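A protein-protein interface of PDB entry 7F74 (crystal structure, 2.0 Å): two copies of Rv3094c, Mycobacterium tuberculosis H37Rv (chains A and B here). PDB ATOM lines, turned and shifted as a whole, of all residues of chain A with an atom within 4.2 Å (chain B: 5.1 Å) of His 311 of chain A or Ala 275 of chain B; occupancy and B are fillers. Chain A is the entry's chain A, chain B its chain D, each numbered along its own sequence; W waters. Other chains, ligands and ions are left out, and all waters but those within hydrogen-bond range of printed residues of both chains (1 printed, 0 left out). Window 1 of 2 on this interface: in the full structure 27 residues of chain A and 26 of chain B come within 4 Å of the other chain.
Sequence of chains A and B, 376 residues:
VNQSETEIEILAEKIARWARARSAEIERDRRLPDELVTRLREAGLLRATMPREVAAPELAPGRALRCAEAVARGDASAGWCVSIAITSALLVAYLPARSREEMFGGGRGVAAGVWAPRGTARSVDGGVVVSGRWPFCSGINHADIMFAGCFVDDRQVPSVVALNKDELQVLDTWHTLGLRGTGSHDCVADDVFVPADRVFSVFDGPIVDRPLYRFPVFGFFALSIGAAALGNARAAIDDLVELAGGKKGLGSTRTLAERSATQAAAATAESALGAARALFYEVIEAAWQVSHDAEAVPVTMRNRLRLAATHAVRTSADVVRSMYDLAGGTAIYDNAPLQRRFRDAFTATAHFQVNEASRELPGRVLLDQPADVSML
The side-chain hydroxyl of Thr 315 of chain A lies within hydrogen-bond range of the backbone carbonyl oxygen of His 311 of chain A (2.8 Å).
The backbone carbonyl oxygen (O) of Thr 268 of chain B lies within hydrogen-bond range of the side-chain hydroxyl (OG) of Ser 271 of chain B, at 3.2 Å.
Printed residues of chain B within 4 Å of Ala 275 of chain A: Ala 275 and Leu 279.
Of chain B, only Ser 271 (3.5 Å), Ala 272 (3.8 Å) and Ala 275 (3.6 Å) come within 4 Å of His 311 of chain A.
Val 313 of chain A touches none of the printed residues of chain B.
Printed residues of chain A within 4 Å of Ala 272 of chain B: His 311 (3.8 Å).
Of the printed residues of chain A, Ala 275 of chain B touches Ala 275 (3.3 Å), Ala 276 (3.98 Å), Leu 279 (3.7 Å) and His 311 (3.6 Å).
The nearest residue of chain B that does not touch His 311 of chain A is Thr 268 of chain B (5.0 Å).
The nearest printed residue of chain A that does not touch Gly 274 of chain B is Ala 275 of chain A (5.4 Å).
Water W1 lies within hydrogen-bond range of ND1 of His 311 of chain A (2.7 Å), OG of Ser 271 of chain B (2.9 Å) and O of Thr 268 of chain B (3.0 Å).
Of the 12 printed residues of chain A, 5 touch a printed residue of chain B.
Hydrophobic or aromatic side chains of chain A within 4 Å of the printed part of chain B: Ala 275, Leu 279 and His 311.
Of the 12 printed residues of chain B, 6 touch a printed residue of chain A.
Among the printed residues, no Asp or Glu carboxylate lies within 4 Å of a Lys or Arg side-chain nitrogen of the other chain.
Ala 275 of chain A touches its own counterpart, Ala 275 of chain B.
Ala 275 of chain A touches Leu 279 of chain B, and with the chains exchanged Leu 279 of chain A touches Ala 275 of chain B.
Ala 276 of chain A touches Ala 275 of chain B, but with the chains exchanged Ala 275 of chain A does not touch Ala 276 of chain B (4.02 Å).
Ala 275 of chain A touches Ala 275 of chain B.
Leu 279 of chain B touches Ala 275 of chain A (CB to CA, 3.6 Å).
Ala 276 of chain A touches Ala 275 of chain B (N to CB, 3.98 Å).
Ser 271 of chain B touches Leu 279 of chain A.
CD1 of Leu 279 of chain A touches C of Gly 274 of chain B (3.9 Å).
Leu 279 of chain A touches Ala 278 of chain B.
Ser 271 of chain B touches Leu 307 of chain A.
OG of Ser 271 of chain B touches ND1 of His 311 of chain A, at 3.5 Å.
Ala 272 of chain B touches His 311 of chain A (CA to CE1, 3.8 Å).
His 311 of chain A touches Ala 275 of chain B (NE2 to CB, 3.6 Å).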
ATOM      1  N   ALA A 275      17.514  19.503   5.902  1.00  0.00           N
ATOM      2  CA  ALA A 275      16.468  20.278   5.239  1.00  0.00           C
ATOM      3  C   ALA A 275      16.349  19.889   3.763  1.00  0.00           C
ATOM      4  O   ALA A 275      15.240  19.662   3.250  1.00  0.00           O
ATOM      5  CB  ALA A 275      16.764  21.763   5.405  1.00  0.00           C
ATOM      6  N   ALA A 276      17.483  19.797   3.069  1.00  0.00           N
ATOM      7  CA  ALA A 276      17.435  19.458   1.651  1.00  0.00           C
ATOM      8  C   ALA A 276      16.847  18.071   1.458  1.00  0.00           C
ATOM      9  O   ALA A 276      16.028  17.857   0.549  1.00  0.00           O
ATOM     10  CB  ALA A 276      18.834  19.556   1.029  1.00  0.00           C
ATOM     11  N   LEU A 279      12.902  18.074   2.038  1.00  0.00           N
ATOM     12  CA  LEU A 279      12.175  18.611   0.911  1.00  0.00           C
ATOM     13  C   LEU A 279      12.180  17.622  -0.244  1.00  0.00           C
ATOM     14  O   LEU A 279      11.141  17.418  -0.879  1.00  0.00           O
ATOM     15  CB  LEU A 279      12.768  19.928   0.470  1.00  0.00           C
ATOM     16  CG  LEU A 279      12.173  20.535  -0.781  1.00  0.00           C
ATOM     17  CD1 LEU A 279      10.769  21.045  -0.520  1.00  0.00           C
ATOM     18  CD2 LEU A 279      13.003  21.646  -1.250  1.00  0.00           C
ATOM     19  N   LEU A 307      13.050  22.064  -8.518  1.00  0.00           N
ATOM     20  CA  LEU A 307      13.534  22.945  -7.457  1.00  0.00           C
ATOM     21  C   LEU A 307      14.271  22.152  -6.387  1.00  0.00           C
ATOM     22  O   LEU A 307      15.393  22.506  -5.988  1.00  0.00           O
ATOM     23  CB  LEU A 307      12.358  23.697  -6.828  1.00  0.00           C
ATOM     24  CG  LEU A 307      11.692  24.767  -7.702  1.00  0.00           C
ATOM     25  CD1 LEU A 307      10.361  25.147  -7.069  1.00  0.00           C
ATOM     26  CD2 LEU A 307      12.634  25.907  -7.886  1.00  0.00           C
ATOM     27  N   ALA A 308      13.618  21.099  -5.887  1.00  0.00           N
ATOM     28  CA  ALA A 308      14.193  20.284  -4.832  1.00  0.00           C
ATOM     29  C   ALA A 308      15.423  19.530  -5.314  1.00  0.00           C
ATOM     30  O   ALA A 308      16.372  19.372  -4.558  1.00  0.00           O
ATOM     31  CB  ALA A 308      13.144  19.315  -4.291  1.00  0.00           C
ATOM     32  N   ALA A 309      15.413  19.036  -6.554  1.00  0.00           N
ATOM     33  CA  ALA A 309      16.591  18.348  -7.079  1.00  0.00           C
ATOM     34  C   ALA A 309      17.817  19.248  -7.116  1.00  0.00           C
ATOM     35  O   ALA A 309      18.918  18.832  -6.732  1.00  0.00           O
ATOM     36  CB  ALA A 309      16.308  17.817  -8.490  1.00  0.00           C
ATOM     37  N   THR A 310      17.669  20.462  -7.665  1.00  0.00           N
ATOM     38  CA  THR A 310      18.796  21.365  -7.756  1.00  0.00           C
ATOM     39  C   THR A 310      19.261  21.799  -6.367  1.00  0.00           C
ATOM     40  O   THR A 310      20.466  21.849  -6.086  1.00  0.00           O
ATOM     41  CB  THR A 310      18.376  22.563  -8.607  1.00  0.00           C
ATOM     42  OG1 THR A 310      18.007  22.076  -9.897  1.00  0.00           O
ATOM     43  CG2 THR A 310      19.509  23.556  -8.733  1.00  0.00           C
ATOM     44  N   HIS A 311      18.320  22.115  -5.480  1.00  0.00           N
ATOM     45  CA  HIS A 311      18.706  22.519  -4.128  1.00  0.00           C
ATOM     46  C   HIS A 311      19.469  21.382  -3.422  1.00  0.00           C
ATOM     47  O   HIS A 311      20.448  21.618  -2.703  1.00  0.00           O
ATOM     48  CB  HIS A 311      17.445  22.874  -3.371  1.00  0.00           C
ATOM     49  CG  HIS A 311      17.691  23.278  -1.970  1.00  0.00           C
ATOM     50  ND1 HIS A 311      18.075  24.556  -1.625  1.00  0.00           N
ATOM     51  CD2 HIS A 311      17.625  22.570  -0.823  1.00  0.00           C
ATOM     52  CE1 HIS A 311      18.203  24.619  -0.307  1.00  0.00           C
ATOM     53  NE2 HIS A 311      17.940  23.430   0.197  1.00  0.00           N
ATOM     54  N   ALA A 312      19.064  20.130  -3.669  1.00  0.00           N
ATOM     55  CA  ALA A 312      19.777  19.001  -3.078  1.00  0.00           C
ATOM     56  C   ALA A 312      21.206  18.893  -3.604  1.00  0.00           C
ATOM     57  O   ALA A 312      22.138  18.670  -2.821  1.00  0.00           O
ATOM     58  CB  ALA A 312      18.990  17.716  -3.337  1.00  0.00           C
ATOM     59  N   VAL A 313      21.424  19.041  -4.921  1.00  0.00           N
ATOM     60  CA  VAL A 313      22.790  18.908  -5.413  1.00  0.00           C
ATOM     61  C   VAL A 313      23.667  20.063  -4.924  1.00  0.00           C
ATOM     62  O   VAL A 313      24.819  19.866  -4.515  1.00  0.00           O
ATOM     63  CB  VAL A 313      22.811  18.798  -6.945  1.00  0.00           C
ATOM     64  CG1 VAL A 313      24.228  18.770  -7.408  1.00  0.00           C
ATOM     65  CG2 VAL A 313      22.081  17.555  -7.344  1.00  0.00           C
ATOM     66  N   ARG A 314      23.144  21.277  -4.939  1.00  0.00           N
ATOM     67  CA  ARG A 314      23.969  22.423  -4.588  1.00  0.00           C
ATOM     68  C   ARG A 314      24.239  22.479  -3.097  1.00  0.00           C
ATOM     69  O   ARG A 314      25.361  22.790  -2.672  1.00  0.00           O
ATOM     70  CB  ARG A 314      23.316  23.733  -5.029  1.00  0.00           C
ATOM     71  CG  ARG A 314      22.705  23.810  -6.378  1.00  0.00           C
ATOM     72  CD  ARG A 314      23.662  24.110  -7.525  1.00  0.00           C
ATOM     73  NE  ARG A 314      24.487  25.337  -7.409  1.00  0.00           N
ATOM     74  CZ  ARG A 314      25.714  25.426  -7.923  1.00  0.00           C
ATOM     75  NH1 ARG A 314      26.218  24.360  -8.549  1.00  0.00           N
ATOM     76  NH2 ARG A 314      26.454  26.528  -7.791  1.00  0.00           N
ATOM     77  N   THR A 315      23.208  22.198  -2.281  1.00  0.00           N
ATOM     78  CA  THR A 315      23.410  22.134  -0.843  1.00  0.00           C
ATOM     79  C   THR A 315      24.383  21.017  -0.459  1.00  0.00           C
ATOM     80  O   THR A 315      25.248  21.206   0.413  1.00  0.00           O
ATOM     81  CB  THR A 315      22.061  21.946  -0.145  1.00  0.00           C
ATOM     82  OG1 THR A 315      21.259  23.108  -0.420  1.00  0.00           O
ATOM     83  CG2 THR A 315      22.266  21.759   1.352  1.00  0.00           C
ATOM     84  N   THR B 268      15.703  29.859  -5.870  1.00  0.00           N
ATOM     85  CA  THR B 268      16.591  29.588  -4.756  1.00  0.00           C
ATOM     86  C   THR B 268      15.836  29.764  -3.443  1.00  0.00           C
ATOM     87  O   THR B 268      15.868  28.896  -2.573  1.00  0.00           O
ATOM     88  CB  THR B 268      17.825  30.492  -4.823  1.00  0.00           C
ATOM     89  OG1 THR B 268      18.569  30.192  -6.022  1.00  0.00           O
ATOM     90  CG2 THR B 268      18.718  30.315  -3.564  1.00  0.00           C
ATOM     91  N   GLU B 270      12.519  29.833  -2.777  1.00  0.00           N
ATOM     92  CA  GLU B 270      11.412  28.896  -2.584  1.00  0.00           C
ATOM     93  C   GLU B 270      11.919  27.519  -2.148  1.00  0.00           C
ATOM     94  O   GLU B 270      11.376  26.897  -1.239  1.00  0.00           O
ATOM     95  CB  GLU B 270      10.621  28.778  -3.873  1.00  0.00           C
ATOM     96  CG  GLU B 270       9.420  27.902  -3.827  1.00  0.00           C
ATOM     97  CD  GLU B 270       8.264  28.592  -3.184  1.00  0.00           C
ATOM     98  OE1 GLU B 270       8.203  29.848  -3.173  1.00  0.00           O
ATOM     99  OE2 GLU B 270       7.420  27.846  -2.678  1.00  0.00           O
ATOM    100  N   SER B 271      12.960  27.023  -2.775  1.00  0.00           N
ATOM    101  CA  SER B 271      13.470  25.723  -2.330  1.00  0.00           C
ATOM    102  C   SER B 271      14.141  25.828  -0.949  1.00  0.00           C
ATOM    103  O   SER B 271      13.983  24.920  -0.110  1.00  0.00           O
ATOM    104  CB  SER B 271      14.376  25.158  -3.422  1.00  0.00           C
ATOM    105  OG  SER B 271      15.547  25.923  -3.630  1.00  0.00           O
ATOM    106  N   ALA B 272      14.850  26.926  -0.663  1.00  0.00           N
ATOM    107  CA  ALA B 272      15.479  27.038   0.652  1.00  0.00           C
ATOM    108  C   ALA B 272      14.424  27.089   1.771  1.00  0.00           C
ATOM    109  O   ALA B 272      14.554  26.398   2.779  1.00  0.00           O
ATOM    110  CB  ALA B 272      16.405  28.258   0.719  1.00  0.00           C
ATOM    111  N   LEU B 273      13.363  27.873   1.586  1.00  0.00           N
ATOM    112  CA  LEU B 273      12.302  27.932   2.577  1.00  0.00           C
ATOM    113  C   LEU B 273      11.614  26.597   2.717  1.00  0.00           C
ATOM    114  O   LEU B 273      11.311  26.153   3.830  1.00  0.00           O
ATOM    115  CB  LEU B 273      11.287  28.995   2.200  1.00  0.00           C
ATOM    116  CG  LEU B 273      10.161  29.159   3.209  1.00  0.00           C
ATOM    117  CD1 LEU B 273      10.690  29.613   4.557  1.00  0.00           C
ATOM    118  CD2 LEU B 273       9.076  30.164   2.703  1.00  0.00           C
ATOM    119  N   GLY B 274      11.265  25.980   1.584  1.00  0.00           N
ATOM    120  CA  GLY B 274      10.585  24.720   1.643  1.00  0.00           C
ATOM    121  C   GLY B 274      11.431  23.668   2.326  1.00  0.00           C
ATOM    122  O   GLY B 274      10.917  22.842   3.084  1.00  0.00           O
ATOM    123  N   ALA B 275      12.739  23.682   2.068  1.00  0.00           N
ATOM    124  CA  ALA B 275      13.613  22.737   2.765  1.00  0.00           C
ATOM    125  C   ALA B 275      13.607  23.003   4.266  1.00  0.00           C
ATOM    126  O   ALA B 275      13.469  22.079   5.083  1.00  0.00           O
ATOM    127  CB  ALA B 275      15.036  22.816   2.203  1.00  0.00           C
ATOM    128  N   ALA B 276      13.702  24.260   4.656  1.00  0.00           N
ATOM    129  CA  ALA B 276      13.699  24.526   6.092  1.00  0.00           C
ATOM    130  C   ALA B 276      12.368  24.124   6.719  1.00  0.00           C
ATOM    131  O   ALA B 276      12.330  23.585   7.827  1.00  0.00           O
ATOM    132  CB  ALA B 276      14.014  26.001   6.337  1.00  0.00           C
ATOM    133  N   ARG B 277      11.260  24.406   6.041  1.00  0.00           N
ATOM    134  CA  ARG B 277       9.943  24.043   6.586  1.00  0.00           C
ATOM    135  C   ARG B 277       9.786  22.529   6.729  1.00  0.00           C
ATOM    136  O   ARG B 277       9.240  22.032   7.725  1.00  0.00           O
ATOM    137  CB  ARG B 277       8.877  24.629   5.666  1.00  0.00           C
ATOM    138  CG  ARG B 277       7.514  24.611   6.144  1.00  0.00           C
ATOM    139  CD  ARG B 277       6.656  25.560   5.333  1.00  0.00           C
ATOM    140  NE  ARG B 277       5.382  25.644   5.999  1.00  0.00           N
ATOM    141  CZ  ARG B 277       4.398  24.796   5.797  1.00  0.00           C
ATOM    142  NH1 ARG B 277       4.555  23.810   4.937  1.00  0.00           N
ATOM    143  NH2 ARG B 277       3.259  24.941   6.449  1.00  0.00           N
ATOM    144  N   ALA B 278      10.333  21.783   5.788  1.00  0.00           N
ATOM    145  CA  ALA B 278      10.176  20.333   5.788  1.00  0.00           C
ATOM    146  C   ALA B 278      10.996  19.705   6.904  1.00  0.00           C
ATOM    147  O   ALA B 278      10.537  18.772   7.581  1.00  0.00           O
ATOM    148  CB  ALA B 278      10.570  19.819   4.397  1.00  0.00           C
ATOM    149  N   LEU B 279      12.191  20.249   7.160  1.00  0.00           N
ATOM    150  CA  LEU B 279      12.972  19.762   8.272  1.00  0.00           C
ATOM    151  C   LEU B 279      12.306  20.112   9.596  1.00  0.00           C
ATOM    152  O   LEU B 279      12.242  19.266  10.487  1.00  0.00           O
ATOM    153  CB  LEU B 279      14.388  20.303   8.221  1.00  0.00           C
ATOM    154  CG  LEU B 279      15.201  19.935   9.441  1.00  0.00           C
ATOM    155  CD1 LEU B 279      15.528  18.438   9.364  1.00  0.00           C
ATOM    156  CD2 LEU B 279      16.431  20.715   9.542  1.00  0.00           C
ATOM    157  N   PHE B 280      11.779  21.346   9.716  1.00  0.00           N
ATOM    158  CA  PHE B 280      11.028  21.802  10.882  1.00  0.00           C
ATOM    159  C   PHE B 280       9.924  20.808  11.269  1.00  0.00           C
ATOM    160  O   PHE B 280       9.902  20.300  12.398  1.00  0.00           O
ATOM    161  CB  PHE B 280      10.495  23.244  10.537  1.00  0.00           C
ATOM    162  CG  PHE B 280       9.788  23.949  11.667  1.00  0.00           C
ATOM    163  CD1 PHE B 280      10.496  24.642  12.611  1.00  0.00           C
ATOM    164  CD2 PHE B 280       8.394  23.986  11.723  1.00  0.00           C
ATOM    165  CE1 PHE B 280       9.843  25.244  13.660  1.00  0.00           C
ATOM    166  CE2 PHE B 280       7.742  24.609  12.736  1.00  0.00           C
ATOM    167  CZ  PHE B 280       8.465  25.247  13.704  1.00  0.00           C
HETATM  168  O   HOH W   1      18.176  26.940  -2.788  1.00  0.00           O
